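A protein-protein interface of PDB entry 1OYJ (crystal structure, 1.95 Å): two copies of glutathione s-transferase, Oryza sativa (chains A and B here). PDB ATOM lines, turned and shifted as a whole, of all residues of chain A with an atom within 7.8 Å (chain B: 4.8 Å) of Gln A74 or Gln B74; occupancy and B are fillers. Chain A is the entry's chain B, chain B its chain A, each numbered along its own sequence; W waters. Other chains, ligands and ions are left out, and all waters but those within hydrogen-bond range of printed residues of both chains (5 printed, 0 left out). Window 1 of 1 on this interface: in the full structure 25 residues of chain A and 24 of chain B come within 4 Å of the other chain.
The guanidinium group of Arg B105 lies within salt-bridge range of the side-chain carboxylate of Asp A78, 3.1 Å away. The guanidinium group (NH2) of Arg A105 lies within salt-bridge range of the side-chain carboxylate (OD1) of Asp B78 (3.2 Å). OD1 of Asp B78 is in salt-bridge range of NE of Arg A101 (3.1 Å). NH1 of Arg B105 sits close to NH1 of Arg A105 (3.2 Å). The guanidinium group of Arg B105 is in hydrogen-bond range of the side-chain amide oxygen of Gln A74.
OE1 of Gln B74 is in hydrogen-bond range of NE of Arg B105 (2.8 Å). O of Leu A70 lies within hydrogen-bond range of NE2 of Gln A74, at 3.4 Å. NE2 of Gln B74 is in hydrogen-bond range of O of Leu B70 (3.5 Å). The guanidinium group (NE) of Arg A105 lies within hydrogen-bond range of the side-chain amide oxygen (OE1) of Gln A74, at 2.8 Å.
Val A71 touches Arg B105 (CG2 to CB, 3.999 Å). OE1 of Gln A74 touches OE1 of Gln B74, at 3.9 Å. Ala A90 touches Asp B78 (CB to OD2, 3.8 Å). Ala A98 touches Tyr B75 (O to CD1, 3.5 Å). Ala A98 touches Asp B78 (CB to C, 3.9 Å). Val B71 touches Ala A102. Ala A102 touches Tyr B75 (CB to CD1, 3.9 Å). Arg A105 touches Gln B74.
Gln A74 touches just these residues of chain B: Gln B74 and Arg B105. Of the printed residues of chain B, Ala A90 touches Asp B78. Of the printed residues of chain B, Ala A98 touches Tyr B75 and Asp B78. Printed residues of chain B within 4 Å of Arg A101: Asp B78 (3.1 Å). Of chain A, only Gln A74 and Arg A105 come within 4 Å of Gln B74. Of the printed residues of chain A, Tyr B75 touches Ala A98 (3.5 Å) and Ala A102 (3.9 Å). Of the printed residues of chain A, Arg B105 touches Val A71, Gln A74, Asp A78 and Arg A105. The nearest residue of chain A that does not touch Gln B74 is Ala A102 (6.6 Å). The nearest printed residue of chain A that does not touch Arg B105 is Arg A101 (4.9 Å).
Along chain B the printed residues that touch a printed residue of chain A span positions 71 to 105. Of the 25 printed residues of chain A, 8 touch a printed residue of chain B. Printed residues of chain A that touch a printed residue of chain B: Val A71, Gln A74, Asp A78, Ala A90, Ala A98, Arg A101, Ala A102 and Arg A105.
Val A71 touches Arg B105, but with the chains exchanged Arg A105 does not touch Val B71 (4.02 Å). Gln A74 touches Arg B105, and with the chains exchanged Arg A105 touches Gln B74. Asp A78 touches Arg B105, and with the chains exchanged Arg A105 touches Asp B78. Arg A105 touches its own counterpart, Arg B105. Positions printed for both chains: 70, 71, 72, 73, 74, 75, 76, 77, 78, 87, 105 and 164. Of the 13 pairs that touch across the chains among the printed residues, 6 have their exchanged pair printed and touching as well.
Water W5 lies within hydrogen-bond range of OD2 of Asp B78, NH2 of Arg A101 and NH1 of Arg A105. Water W4 lies within hydrogen-bond range of the side-chain carboxylate (OD1) of Asp B78 and the backbone carbonyl oxygen (O) of Ala A98. Water W1 lies within hydrogen-bond range of O of Val A71 (2.9 Å), NH2 of Arg B105 (3.2 Å) and N of Tyr A75 (3.5 Å). Water W2 bridges NH2 of Arg A105 (3.0 Å) and O of Val B71 (3.0 Å).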
ATOM      1  N   ALA A  24       7.362  11.673 -12.059  1.00  0.00           N
ATOM      2  CA  ALA A  24       8.637  12.360 -12.217  1.00  0.00           C
ATOM      3  C   ALA A  24       9.286  11.969 -13.524  1.00  0.00           C
ATOM      4  O   ALA A  24       9.801  12.830 -14.221  1.00  0.00           O
ATOM      5  CB  ALA A  24       9.554  12.071 -11.152  1.00  0.00           C
ATOM      6  N   LYS A  28       9.947  14.142 -16.958  1.00  0.00           N
ATOM      7  CA  LYS A  28      11.287  14.267 -17.517  1.00  0.00           C
ATOM      8  C   LYS A  28      11.462  13.659 -18.900  1.00  0.00           C
ATOM      9  O   LYS A  28      12.557  13.718 -19.415  1.00  0.00           O
ATOM     10  CB  LYS A  28      12.317  13.661 -16.554  1.00  0.00           C
ATOM     11  CG  LYS A  28      12.560  14.511 -15.298  1.00  0.00           C
ATOM     12  CD  LYS A  28      13.258  13.804 -14.119  1.00  0.00           C
ATOM     13  CE  LYS A  28      13.628  14.796 -13.022  1.00  0.00           C
ATOM     14  NZ  LYS A  28      14.724  15.734 -13.324  1.00  0.00           N
ATOM     15  N   VAL A  66      17.728   2.103  -6.535  1.00  0.00           N
ATOM     16  CA  VAL A  66      17.617   3.293  -5.739  1.00  0.00           C
ATOM     17  C   VAL A  66      16.227   3.167  -5.063  1.00  0.00           C
ATOM     18  O   VAL A  66      15.231   2.967  -5.739  1.00  0.00           O
ATOM     19  CB  VAL A  66      17.694   4.535  -6.623  1.00  0.00           C
ATOM     20  CG1 VAL A  66      17.492   5.759  -5.771  1.00  0.00           C
ATOM     21  CG2 VAL A  66      18.975   4.609  -7.352  1.00  0.00           C
ATOM     22  N   GLU A  68      13.352   4.425  -1.696  1.00  0.00           N
ATOM     23  CA  GLU A  68      12.815   5.589  -0.991  1.00  0.00           C
ATOM     24  C   GLU A  68      12.448   6.628  -2.063  1.00  0.00           C
ATOM     25  O   GLU A  68      13.296   7.233  -2.719  1.00  0.00           O
ATOM     26  CB  GLU A  68      13.714   6.147   0.109  1.00  0.00           C
ATOM     27  CG  GLU A  68      13.861   5.218   1.312  1.00  0.00           C
ATOM     28  CD  GLU A  68      12.517   4.952   2.048  1.00  0.00           C
ATOM     29  OE1 GLU A  68      11.796   5.911   2.295  1.00  0.00           O
ATOM     30  OE2 GLU A  68      12.159   3.773   2.311  1.00  0.00           O
ATOM     31  N   SER A  69      11.127   6.816  -2.188  1.00  0.00           N
ATOM     32  CA  SER A  69      10.561   7.642  -3.220  1.00  0.00           C
ATOM     33  C   SER A  69      11.171   9.032  -3.245  1.00  0.00           C
ATOM     34  O   SER A  69      11.456   9.490  -4.347  1.00  0.00           O
ATOM     35  CB  SER A  69       8.998   7.664  -3.155  1.00  0.00           C
ATOM     36  OG  SER A  69       8.507   8.336  -2.029  1.00  0.00           O
ATOM     37  N   LEU A  70      11.377   9.699  -2.095  1.00  0.00           N
ATOM     38  CA  LEU A  70      11.999  11.064  -2.163  1.00  0.00           C
ATOM     39  C   LEU A  70      13.449  11.042  -2.629  1.00  0.00           C
ATOM     40  O   LEU A  70      13.916  11.970  -3.288  1.00  0.00           O
ATOM     41  CB  LEU A  70      11.837  11.847  -0.855  1.00  0.00           C
ATOM     42  CG  LEU A  70      10.381  12.172  -0.531  1.00  0.00           C
ATOM     43  CD1 LEU A  70      10.380  13.025   0.696  1.00  0.00           C
ATOM     44  CD2 LEU A  70       9.731  12.936  -1.711  1.00  0.00           C
ATOM     45  N   VAL A  71      14.132   9.959  -2.289  1.00  0.00           N
ATOM     46  CA  VAL A  71      15.484   9.676  -2.723  1.00  0.00           C
ATOM     47  C   VAL A  71      15.520   9.488  -4.281  1.00  0.00           C
ATOM     48  O   VAL A  71      16.364  10.039  -4.959  1.00  0.00           O
ATOM     49  CB  VAL A  71      16.116   8.489  -1.954  1.00  0.00           C
ATOM     50  CG1 VAL A  71      17.585   8.134  -2.445  1.00  0.00           C
ATOM     51  CG2 VAL A  71      16.204   8.779  -0.482  1.00  0.00           C
ATOM     52  N   ILE A  72      14.563   8.715  -4.792  1.00  0.00           N
ATOM     53  CA  ILE A  72      14.426   8.449  -6.186  1.00  0.00           C
ATOM     54  C   ILE A  72      14.169   9.739  -6.941  1.00  0.00           C
ATOM     55  O   ILE A  72      14.738   9.983  -7.987  1.00  0.00           O
ATOM     56  CB  ILE A  72      13.284   7.425  -6.426  1.00  0.00           C
ATOM     57  CG1 ILE A  72      13.711   6.036  -5.941  1.00  0.00           C
ATOM     58  CG2 ILE A  72      13.057   7.301  -7.918  1.00  0.00           C
ATOM     59  CD1 ILE A  72      12.564   5.103  -5.782  1.00  0.00           C
ATOM     60  N   LEU A  73      13.275  10.568  -6.424  1.00  0.00           N
ATOM     61  CA  LEU A  73      13.052  11.829  -7.086  1.00  0.00           C
ATOM     62  C   LEU A  73      14.308  12.658  -7.202  1.00  0.00           C
ATOM     63  O   LEU A  73      14.560  13.156  -8.267  1.00  0.00           O
ATOM     64  CB  LEU A  73      12.028  12.661  -6.401  1.00  0.00           C
ATOM     65  CG  LEU A  73      10.619  12.137  -6.303  1.00  0.00           C
ATOM     66  CD1 LEU A  73       9.691  13.239  -5.824  1.00  0.00           C
ATOM     67  CD2 LEU A  73      10.087  11.612  -7.536  1.00  0.00           C
ATOM     68  N   GLN A  74      15.125  12.730  -6.161  1.00  0.00           N
ATOM     69  CA  GLN A  74      16.325  13.496  -6.227  1.00  0.00           C
ATOM     70  C   GLN A  74      17.375  12.852  -7.153  1.00  0.00           C
ATOM     71  O   GLN A  74      18.167  13.534  -7.816  1.00  0.00           O
ATOM     72  CB  GLN A  74      16.871  13.758  -4.804  1.00  0.00           C
ATOM     73  CG  GLN A  74      15.977  14.690  -3.950  1.00  0.00           C
ATOM     74  CD  GLN A  74      16.479  14.900  -2.535  1.00  0.00           C
ATOM     75  OE1 GLN A  74      17.187  15.843  -2.297  1.00  0.00           O
ATOM     76  NE2 GLN A  74      16.096  14.049  -1.610  1.00  0.00           N
ATOM     77  N   TYR A  75      17.363  11.549  -7.195  1.00  0.00           N
ATOM     78  CA  TYR A  75      18.239  10.786  -8.081  1.00  0.00           C
ATOM     79  C   TYR A  75      17.913  11.149  -9.549  1.00  0.00           C
ATOM     80  O   TYR A  75      18.815  11.354 -10.333  1.00  0.00           O
ATOM     81  CB  TYR A  75      18.032   9.310  -7.900  1.00  0.00           C
ATOM     82  CG  TYR A  75      18.864   8.505  -8.838  1.00  0.00           C
ATOM     83  CD1 TYR A  75      20.215   8.372  -8.587  1.00  0.00           C
ATOM     84  CD2 TYR A  75      18.326   7.921 -10.003  1.00  0.00           C
ATOM     85  CE1 TYR A  75      21.059   7.723  -9.458  1.00  0.00           C
ATOM     86  CE2 TYR A  75      19.174   7.187 -10.850  1.00  0.00           C
ATOM     87  CZ  TYR A  75      20.523   7.097 -10.587  1.00  0.00           C
ATOM     88  OH  TYR A  75      21.403   6.387 -11.455  1.00  0.00           O
ATOM     89  N   LEU A  76      16.618  11.206  -9.875  1.00  0.00           N
ATOM     90  CA  LEU A  76      16.195  11.516 -11.238  1.00  0.00           C
ATOM     91  C   LEU A  76      16.669  12.932 -11.681  1.00  0.00           C
ATOM     92  O   LEU A  76      16.864  13.171 -12.850  1.00  0.00           O
ATOM     93  CB  LEU A  76      14.704  11.421 -11.396  1.00  0.00           C
ATOM     94  CG  LEU A  76      14.196   9.987 -11.293  1.00  0.00           C
ATOM     95  CD1 LEU A  76      12.752  10.020 -11.175  1.00  0.00           C
ATOM     96  CD2 LEU A  76      14.652   9.050 -12.447  1.00  0.00           C
ATOM     97  N   ASP A  77      16.784  13.885 -10.778  1.00  0.00           N
ATOM     98  CA  ASP A  77      17.378  15.185 -11.167  1.00  0.00           C
ATOM     99  C   ASP A  77      18.898  14.972 -11.352  1.00  0.00           C
ATOM    100  O   ASP A  77      19.523  15.368 -12.361  1.00  0.00           O
ATOM    101  CB  ASP A  77      17.291  16.183 -10.036  1.00  0.00           C
ATOM    102  CG  ASP A  77      16.054  17.030 -10.063  1.00  0.00           C
ATOM    103  OD1 ASP A  77      15.165  16.836 -10.926  1.00  0.00           O
ATOM    104  OD2 ASP A  77      15.913  17.933  -9.207  1.00  0.00           O
ATOM    105  N   ASP A  78      19.515  14.405 -10.301  1.00  0.00           N
ATOM    106  CA  ASP A  78      20.969  14.228 -10.260  1.00  0.00           C
ATOM    107  C   ASP A  78      21.531  13.396 -11.435  1.00  0.00           C
ATOM    108  O   ASP A  78      22.627  13.649 -11.903  1.00  0.00           O
ATOM    109  CB  ASP A  78      21.437  13.501  -8.976  1.00  0.00           C
ATOM    110  CG  ASP A  78      21.395  14.396  -7.712  1.00  0.00           C
ATOM    111  OD1 ASP A  78      21.508  13.887  -6.559  1.00  0.00           O
ATOM    112  OD2 ASP A  78      21.178  15.611  -7.802  1.00  0.00           O
ATOM    113  N   ALA A  79      20.798  12.391 -11.864  1.00  0.00           N
ATOM    114  CA  ALA A  79      21.304  11.447 -12.828  1.00  0.00           C
ATOM    115  C   ALA A  79      20.928  11.848 -14.220  1.00  0.00           C
ATOM    116  O   ALA A  79      21.505  11.308 -15.188  1.00  0.00           O
ATOM    117  CB  ALA A  79      20.747  10.040 -12.521  1.00  0.00           C
ATOM    118  N   PHE A  80      20.033  12.817 -14.337  1.00  0.00           N
ATOM    119  CA  PHE A  80      19.535  13.238 -15.648  1.00  0.00           C
ATOM    120  C   PHE A  80      19.462  14.748 -15.673  1.00  0.00           C
ATOM    121  O   PHE A  80      18.380  15.345 -15.775  1.00  0.00           O
ATOM    122  CB  PHE A  80      18.154  12.630 -15.869  1.00  0.00           C
ATOM    123  CG  PHE A  80      18.164  11.159 -15.953  1.00  0.00           C
ATOM    124  CD1 PHE A  80      17.725  10.380 -14.885  1.00  0.00           C
ATOM    125  CD2 PHE A  80      18.622  10.525 -17.091  1.00  0.00           C
ATOM    126  CE1 PHE A  80      17.729   9.028 -14.975  1.00  0.00           C
ATOM    127  CE2 PHE A  80      18.646   9.156 -17.174  1.00  0.00           C
ATOM    128  CZ  PHE A  80      18.200   8.404 -16.107  1.00  0.00           C
ATOM    129  N   LEU A  86      13.230  18.945 -10.740  1.00  0.00           N
ATOM    130  CA  LEU A  86      12.241  19.068  -9.636  1.00  0.00           C
ATOM    131  C   LEU A  86      12.706  20.040  -8.555  1.00  0.00           C
ATOM    132  O   LEU A  86      11.873  20.689  -7.890  1.00  0.00           O
ATOM    133  CB  LEU A  86      11.946  17.757  -8.984  1.00  0.00           C
ATOM    134  CG  LEU A  86      11.319  16.750  -9.946  1.00  0.00           C
ATOM    135  CD1 LEU A  86      11.341  15.330  -9.319  1.00  0.00           C
ATOM    136  CD2 LEU A  86       9.985  17.094 -10.313  1.00  0.00           C
ATOM    137  N   LEU A  87      14.005  20.173  -8.411  1.00  0.00           N
ATOM    138  CA  LEU A  87      14.564  21.135  -7.438  1.00  0.00           C
ATOM    139  C   LEU A  87      15.475  22.074  -8.207  1.00  0.00           C
ATOM    140  O   LEU A  87      16.157  21.623  -9.109  1.00  0.00           O
ATOM    141  CB  LEU A  87      15.382  20.399  -6.390  1.00  0.00           C
ATOM    142  CG  LEU A  87      14.524  19.596  -5.397  1.00  0.00           C
ATOM    143  CD1 LEU A  87      15.383  18.591  -4.758  1.00  0.00           C
ATOM    144  CD2 LEU A  87      13.926  20.445  -4.333  1.00  0.00           C
ATOM    145  N   ALA A  90      21.431  24.154  -7.218  1.00  0.00           N
ATOM    146  CA  ALA A  90      22.117  24.988  -6.229  1.00  0.00           C
ATOM    147  C   ALA A  90      23.102  25.956  -6.846  1.00  0.00           C
ATOM    148  O   ALA A  90      22.985  27.157  -6.635  1.00  0.00           O
ATOM    149  CB  ALA A  90      22.829  24.103  -5.188  1.00  0.00           C
ATOM    150  N   ALA A  98      19.543  27.662  -2.831  1.00  0.00           N
ATOM    151  CA  ALA A  98      19.899  26.848  -1.689  1.00  0.00           C
ATOM    152  C   ALA A  98      18.727  26.809  -0.719  1.00  0.00           C
ATOM    153  O   ALA A  98      18.312  25.765  -0.283  1.00  0.00           O
ATOM    154  CB  ALA A  98      21.154  27.468  -1.007  1.00  0.00           C
ATOM    155  N   ARG A 101      15.627  24.995  -2.127  1.00  0.00           N
ATOM    156  CA  ARG A 101      15.759  23.601  -2.008  1.00  0.00           C
ATOM    157  C   ARG A 101      15.480  23.079  -0.632  1.00  0.00           C
ATOM    158  O   ARG A 101      14.924  21.970  -0.479  1.00  0.00           O
ATOM    159  CB  ARG A 101      17.191  23.191  -2.389  1.00  0.00           C
ATOM    160  CG  ARG A 101      17.450  23.281  -3.860  1.00  0.00           C
ATOM    161  CD  ARG A 101      18.911  23.237  -4.314  1.00  0.00           C
ATOM    162  NE  ARG A 101      19.537  21.938  -4.261  1.00  0.00           N
ATOM    163  CZ  ARG A 101      19.594  21.117  -5.290  1.00  0.00           C
ATOM    164  NH1 ARG A 101      19.034  21.490  -6.427  1.00  0.00           N
ATOM    165  NH2 ARG A 101      20.238  19.952  -5.217  1.00  0.00           N
ATOM    166  N   ALA A 102      15.992  23.769   0.383  1.00  0.00           N
ATOM    167  CA  ALA A 102      15.734  23.323   1.729  1.00  0.00           C
ATOM    168  C   ALA A 102      14.271  23.391   2.029  1.00  0.00           C
ATOM    169  O   ALA A 102      13.697  22.456   2.545  1.00  0.00           O
ATOM    170  CB  ALA A 102      16.535  24.185   2.719  1.00  0.00           C
ATOM    171  N   ARG A 105      12.625  20.400   0.369  1.00  0.00           N
ATOM    172  CA  ARG A 105      12.852  19.167   1.055  1.00  0.00           C
ATOM    173  C   ARG A 105      12.034  19.080   2.350  1.00  0.00           C
ATOM    174  O   ARG A 105      11.552  18.043   2.701  1.00  0.00           O
ATOM    175  CB  ARG A 105      14.323  19.030   1.372  1.00  0.00           C
ATOM    176  CG  ARG A 105      15.141  18.819   0.122  1.00  0.00           C
ATOM    177  CD  ARG A 105      16.539  18.577   0.407  1.00  0.00           C
ATOM    178  NE  ARG A 105      17.292  18.197  -0.762  1.00  0.00           N
ATOM    179  CZ  ARG A 105      18.320  18.830  -1.232  1.00  0.00           C
ATOM    180  NH1 ARG A 105      18.907  18.392  -2.322  1.00  0.00           N
ATOM    181  NH2 ARG A 105      18.774  19.906  -0.636  1.00  0.00           N
ATOM    182  N   ALA A 108       8.415  18.266   1.435  1.00  0.00           N
ATOM    183  CA  ALA A 108       8.254  16.910   0.974  1.00  0.00           C
ATOM    184  C   ALA A 108       8.321  15.950   2.157  1.00  0.00           C
ATOM    185  O   ALA A 108       7.484  15.054   2.263  1.00  0.00           O
ATOM    186  CB  ALA A 108       9.346  16.612  -0.116  1.00  0.00           C
ATOM    187  N   PHE A 164       9.375  19.552  -6.902  1.00  0.00           N
ATOM    188  CA  PHE A 164       9.574  18.501  -5.968  1.00  0.00           C
ATOM    189  C   PHE A 164       8.385  18.303  -5.084  1.00  0.00           C
ATOM    190  O   PHE A 164       7.843  17.227  -5.018  1.00  0.00           O
ATOM    191  CB  PHE A 164      10.790  18.859  -5.140  1.00  0.00           C
ATOM    192  CG  PHE A 164      11.292  17.785  -4.314  1.00  0.00           C
ATOM    193  CD1 PHE A 164      11.791  16.626  -4.887  1.00  0.00           C
ATOM    194  CD2 PHE A 164      11.288  17.890  -2.947  1.00  0.00           C
ATOM    195  CE1 PHE A 164      12.321  15.628  -4.110  1.00  0.00           C
ATOM    196  CE2 PHE A 164      11.854  16.886  -2.178  1.00  0.00           C
ATOM    197  CZ  PHE A 164      12.338  15.781  -2.705  1.00  0.00           C
ATOM    198  N   LEU B  70      18.448  16.753   8.732  1.00  0.00           N
ATOM    199  CA  LEU B  70      19.066  16.277   7.468  1.00  0.00           C
ATOM    200  C   LEU B  70      18.912  17.301   6.333  1.00  0.00           C
ATOM    201  O   LEU B  70      19.731  17.375   5.408  1.00  0.00           O
ATOM    202  CB  LEU B  70      18.475  14.926   7.032  1.00  0.00           C
ATOM    203  CG  LEU B  70      18.819  13.699   7.862  1.00  0.00           C
ATOM    204  CD1 LEU B  70      18.291  12.371   7.248  1.00  0.00           C
ATOM    205  CD2 LEU B  70      20.282  13.565   8.035  1.00  0.00           C
ATOM    206  N   VAL B  71      17.866  18.097   6.450  1.00  0.00           N
ATOM    207  CA  VAL B  71      17.613  19.190   5.550  1.00  0.00           C
ATOM    208  C   VAL B  71      18.701  20.288   5.784  1.00  0.00           C
ATOM    209  O   VAL B  71      19.273  20.802   4.819  1.00  0.00           O
ATOM    210  CB  VAL B  71      16.114  19.751   5.696  1.00  0.00           C
ATOM    211  CG1 VAL B  71      15.934  21.038   4.810  1.00  0.00           C
ATOM    212  CG2 VAL B  71      15.104  18.714   5.305  1.00  0.00           C
ATOM    213  N   ILE B  72      18.994  20.616   7.059  1.00  0.00           N
ATOM    214  CA  ILE B  72      20.006  21.592   7.412  1.00  0.00           C
ATOM    215  C   ILE B  72      21.380  21.100   6.883  1.00  0.00           C
ATOM    216  O   ILE B  72      22.099  21.849   6.269  1.00  0.00           O
ATOM    217  CB  ILE B  72      20.064  21.817   8.993  1.00  0.00           C
ATOM    218  CG1 ILE B  72      18.787  22.506   9.543  1.00  0.00           C
ATOM    219  CG2 ILE B  72      21.280  22.538   9.319  1.00  0.00           C
ATOM    220  CD1 ILE B  72      18.503  22.218  10.986  1.00  0.00           C
ATOM    221  N   LEU B  73      21.688  19.817   7.078  1.00  0.00           N
ATOM    222  CA  LEU B  73      22.948  19.272   6.541  1.00  0.00           C
ATOM    223  C   LEU B  73      23.072  19.483   5.005  1.00  0.00           C
ATOM    224  O   LEU B  73      24.097  19.984   4.518  1.00  0.00           O
ATOM    225  CB  LEU B  73      23.098  17.836   6.841  1.00  0.00           C
ATOM    226  CG  LEU B  73      23.220  17.376   8.263  1.00  0.00           C
ATOM    227  CD1 LEU B  73      23.755  15.938   8.286  1.00  0.00           C
ATOM    228  CD2 LEU B  73      24.079  18.277   9.037  1.00  0.00           C
ATOM    229  N   GLN B  74      22.044  19.195   4.259  1.00  0.00           N
ATOM    230  CA  GLN B  74      22.119  19.400   2.826  1.00  0.00           C
ATOM    231  C   GLN B  74      22.202  20.856   2.460  1.00  0.00           C
ATOM    232  O   GLN B  74      22.949  21.276   1.515  1.00  0.00           O
ATOM    233  CB  GLN B  74      20.940  18.723   2.180  1.00  0.00           C
ATOM    234  CG  GLN B  74      21.122  17.217   2.207  1.00  0.00           C
ATOM    235  CD  GLN B  74      19.983  16.526   1.508  1.00  0.00           C
ATOM    236  OE1 GLN B  74      20.069  16.246   0.344  1.00  0.00           O
ATOM    237  NE2 GLN B  74      18.920  16.266   2.233  1.00  0.00           N
ATOM    238  N   TYR B  75      21.557  21.652   3.302  1.00  0.00           N
ATOM    239  CA  TYR B  75      21.609  23.093   3.127  1.00  0.00           C
ATOM    240  C   TYR B  75      23.028  23.632   3.300  1.00  0.00           C
ATOM    241  O   TYR B  75      23.490  24.505   2.530  1.00  0.00           O
ATOM    242  CB  TYR B  75      20.561  23.809   4.009  1.00  0.00           C
ATOM    243  CG  TYR B  75      20.557  25.337   3.906  1.00  0.00           C
ATOM    244  CD1 TYR B  75      20.015  25.974   2.801  1.00  0.00           C
ATOM    245  CD2 TYR B  75      21.184  26.126   4.873  1.00  0.00           C
ATOM    246  CE1 TYR B  75      20.039  27.381   2.697  1.00  0.00           C
ATOM    247  CE2 TYR B  75      21.226  27.507   4.769  1.00  0.00           C
ATOM    248  CZ  TYR B  75      20.652  28.130   3.692  1.00  0.00           C
ATOM    249  OH  TYR B  75      20.690  29.498   3.625  1.00  0.00           O
ATOM    250  N   LEU B  76      23.729  23.136   4.300  1.00  0.00           N
ATOM    251  CA  LEU B  76      25.086  23.567   4.572  1.00  0.00           C
ATOM    252  C   LEU B  76      26.008  23.244   3.372  1.00  0.00           C
ATOM    253  O   LEU B  76      27.011  23.957   3.177  1.00  0.00           O
ATOM    254  CB  LEU B  76      25.615  22.996   5.855  1.00  0.00           C
ATOM    255  CG  LEU B  76      24.888  23.484   7.100  1.00  0.00           C
ATOM    256  CD1 LEU B  76      25.413  22.679   8.359  1.00  0.00           C
ATOM    257  CD2 LEU B  76      25.130  24.943   7.249  1.00  0.00           C
ATOM    258  N   ASP B  77      25.727  22.197   2.591  1.00  0.00           N
ATOM    259  CA  ASP B  77      26.466  22.009   1.348  1.00  0.00           C
ATOM    260  C   ASP B  77      25.951  23.044   0.312  1.00  0.00           C
ATOM    261  O   ASP B  77      26.757  23.770  -0.328  1.00  0.00           O
ATOM    262  CB  ASP B  77      26.213  20.673   0.688  1.00  0.00           C
ATOM    263  CG  ASP B  77      27.140  19.565   1.163  1.00  0.00           C
ATOM    264  OD1 ASP B  77      28.063  19.815   2.012  1.00  0.00           O
ATOM    265  OD2 ASP B  77      26.992  18.412   0.694  1.00  0.00           O
ATOM    266  N   ASP B  78      24.627  23.122   0.145  1.00  0.00           N
ATOM    267  CA  ASP B  78      24.090  23.924  -0.963  1.00  0.00           C
ATOM    268  C   ASP B  78      24.420  25.370  -0.801  1.00  0.00           C
ATOM    269  O   ASP B  78      24.745  26.054  -1.760  1.00  0.00           O
ATOM    270  CB  ASP B  78      22.563  23.794  -1.130  1.00  0.00           C
ATOM    271  CG  ASP B  78      22.121  22.436  -1.642  1.00  0.00           C
ATOM    272  OD1 ASP B  78      20.911  22.139  -1.448  1.00  0.00           O
ATOM    273  OD2 ASP B  78      22.889  21.628  -2.240  1.00  0.00           O
ATOM    274  N   LEU B  87      28.099  15.630   0.834  1.00  0.00           N
ATOM    275  CA  LEU B  87      27.697  14.773  -0.262  1.00  0.00           C
ATOM    276  C   LEU B  87      28.520  15.172  -1.461  1.00  0.00           C
ATOM    277  O   LEU B  87      28.844  16.328  -1.635  1.00  0.00           O
ATOM    278  CB  LEU B  87      26.230  14.990  -0.564  1.00  0.00           C
ATOM    279  CG  LEU B  87      25.229  14.540   0.498  1.00  0.00           C
ATOM    280  CD1 LEU B  87      23.912  15.137   0.272  1.00  0.00           C
ATOM    281  CD2 LEU B  87      25.167  13.092   0.514  1.00  0.00           C
ATOM    282  N   ARG B 105      21.729   9.416   0.884  1.00  0.00           N
ATOM    283  CA  ARG B 105      20.443   9.826   1.399  1.00  0.00           C
ATOM    284  C   ARG B 105      19.645   8.657   1.929  1.00  0.00           C
ATOM    285  O   ARG B 105      18.991   8.797   2.922  1.00  0.00           O
ATOM    286  CB  ARG B 105      19.609  10.652   0.462  1.00  0.00           C
ATOM    287  CG  ARG B 105      20.300  11.941  -0.074  1.00  0.00           C
ATOM    288  CD  ARG B 105      19.425  12.682  -1.165  1.00  0.00           C
ATOM    289  NE  ARG B 105      19.862  14.061  -1.426  1.00  0.00           N
ATOM    290  CZ  ARG B 105      20.267  14.542  -2.582  1.00  0.00           C
ATOM    291  NH1 ARG B 105      20.722  15.785  -2.617  1.00  0.00           N
ATOM    292  NH2 ARG B 105      20.218  13.838  -3.706  1.00  0.00           N
ATOM    293  N   PHE B 164      28.189  12.784   4.695  1.00  0.00           N
ATOM    294  CA  PHE B 164      26.768  12.891   5.085  1.00  0.00           C
ATOM    295  C   PHE B 164      26.256  11.827   6.064  1.00  0.00           C
ATOM    296  O   PHE B 164      25.727  12.140   7.104  1.00  0.00           O
ATOM    297  CB  PHE B 164      25.914  12.844   3.845  1.00  0.00           C
ATOM    298  CG  PHE B 164      24.489  13.258   4.037  1.00  0.00           C
ATOM    299  CD1 PHE B 164      24.155  14.503   4.426  1.00  0.00           C
ATOM    300  CD2 PHE B 164      23.456  12.414   3.681  1.00  0.00           C
ATOM    301  CE1 PHE B 164      22.782  14.871   4.550  1.00  0.00           C
ATOM    302  CE2 PHE B 164      22.104  12.826   3.705  1.00  0.00           C
ATOM    303  CZ  PHE B 164      21.781  14.010   4.214  1.00  0.00           C
HETATM  304  O   HOH W   1      19.091  10.919  -4.265  1.00  0.00           O
HETATM  305  O   HOH W   2      18.265  21.188   1.987  1.00  0.00           O
HETATM  306  O   HOH W   3      21.053  16.361  -5.269  1.00  0.00           O
HETATM  307  O   HOH W   4      19.884  23.585   0.839  1.00  0.00           O
HETATM  308  O   HOH W   5      21.727  19.288  -2.794  1.00  0.00           O
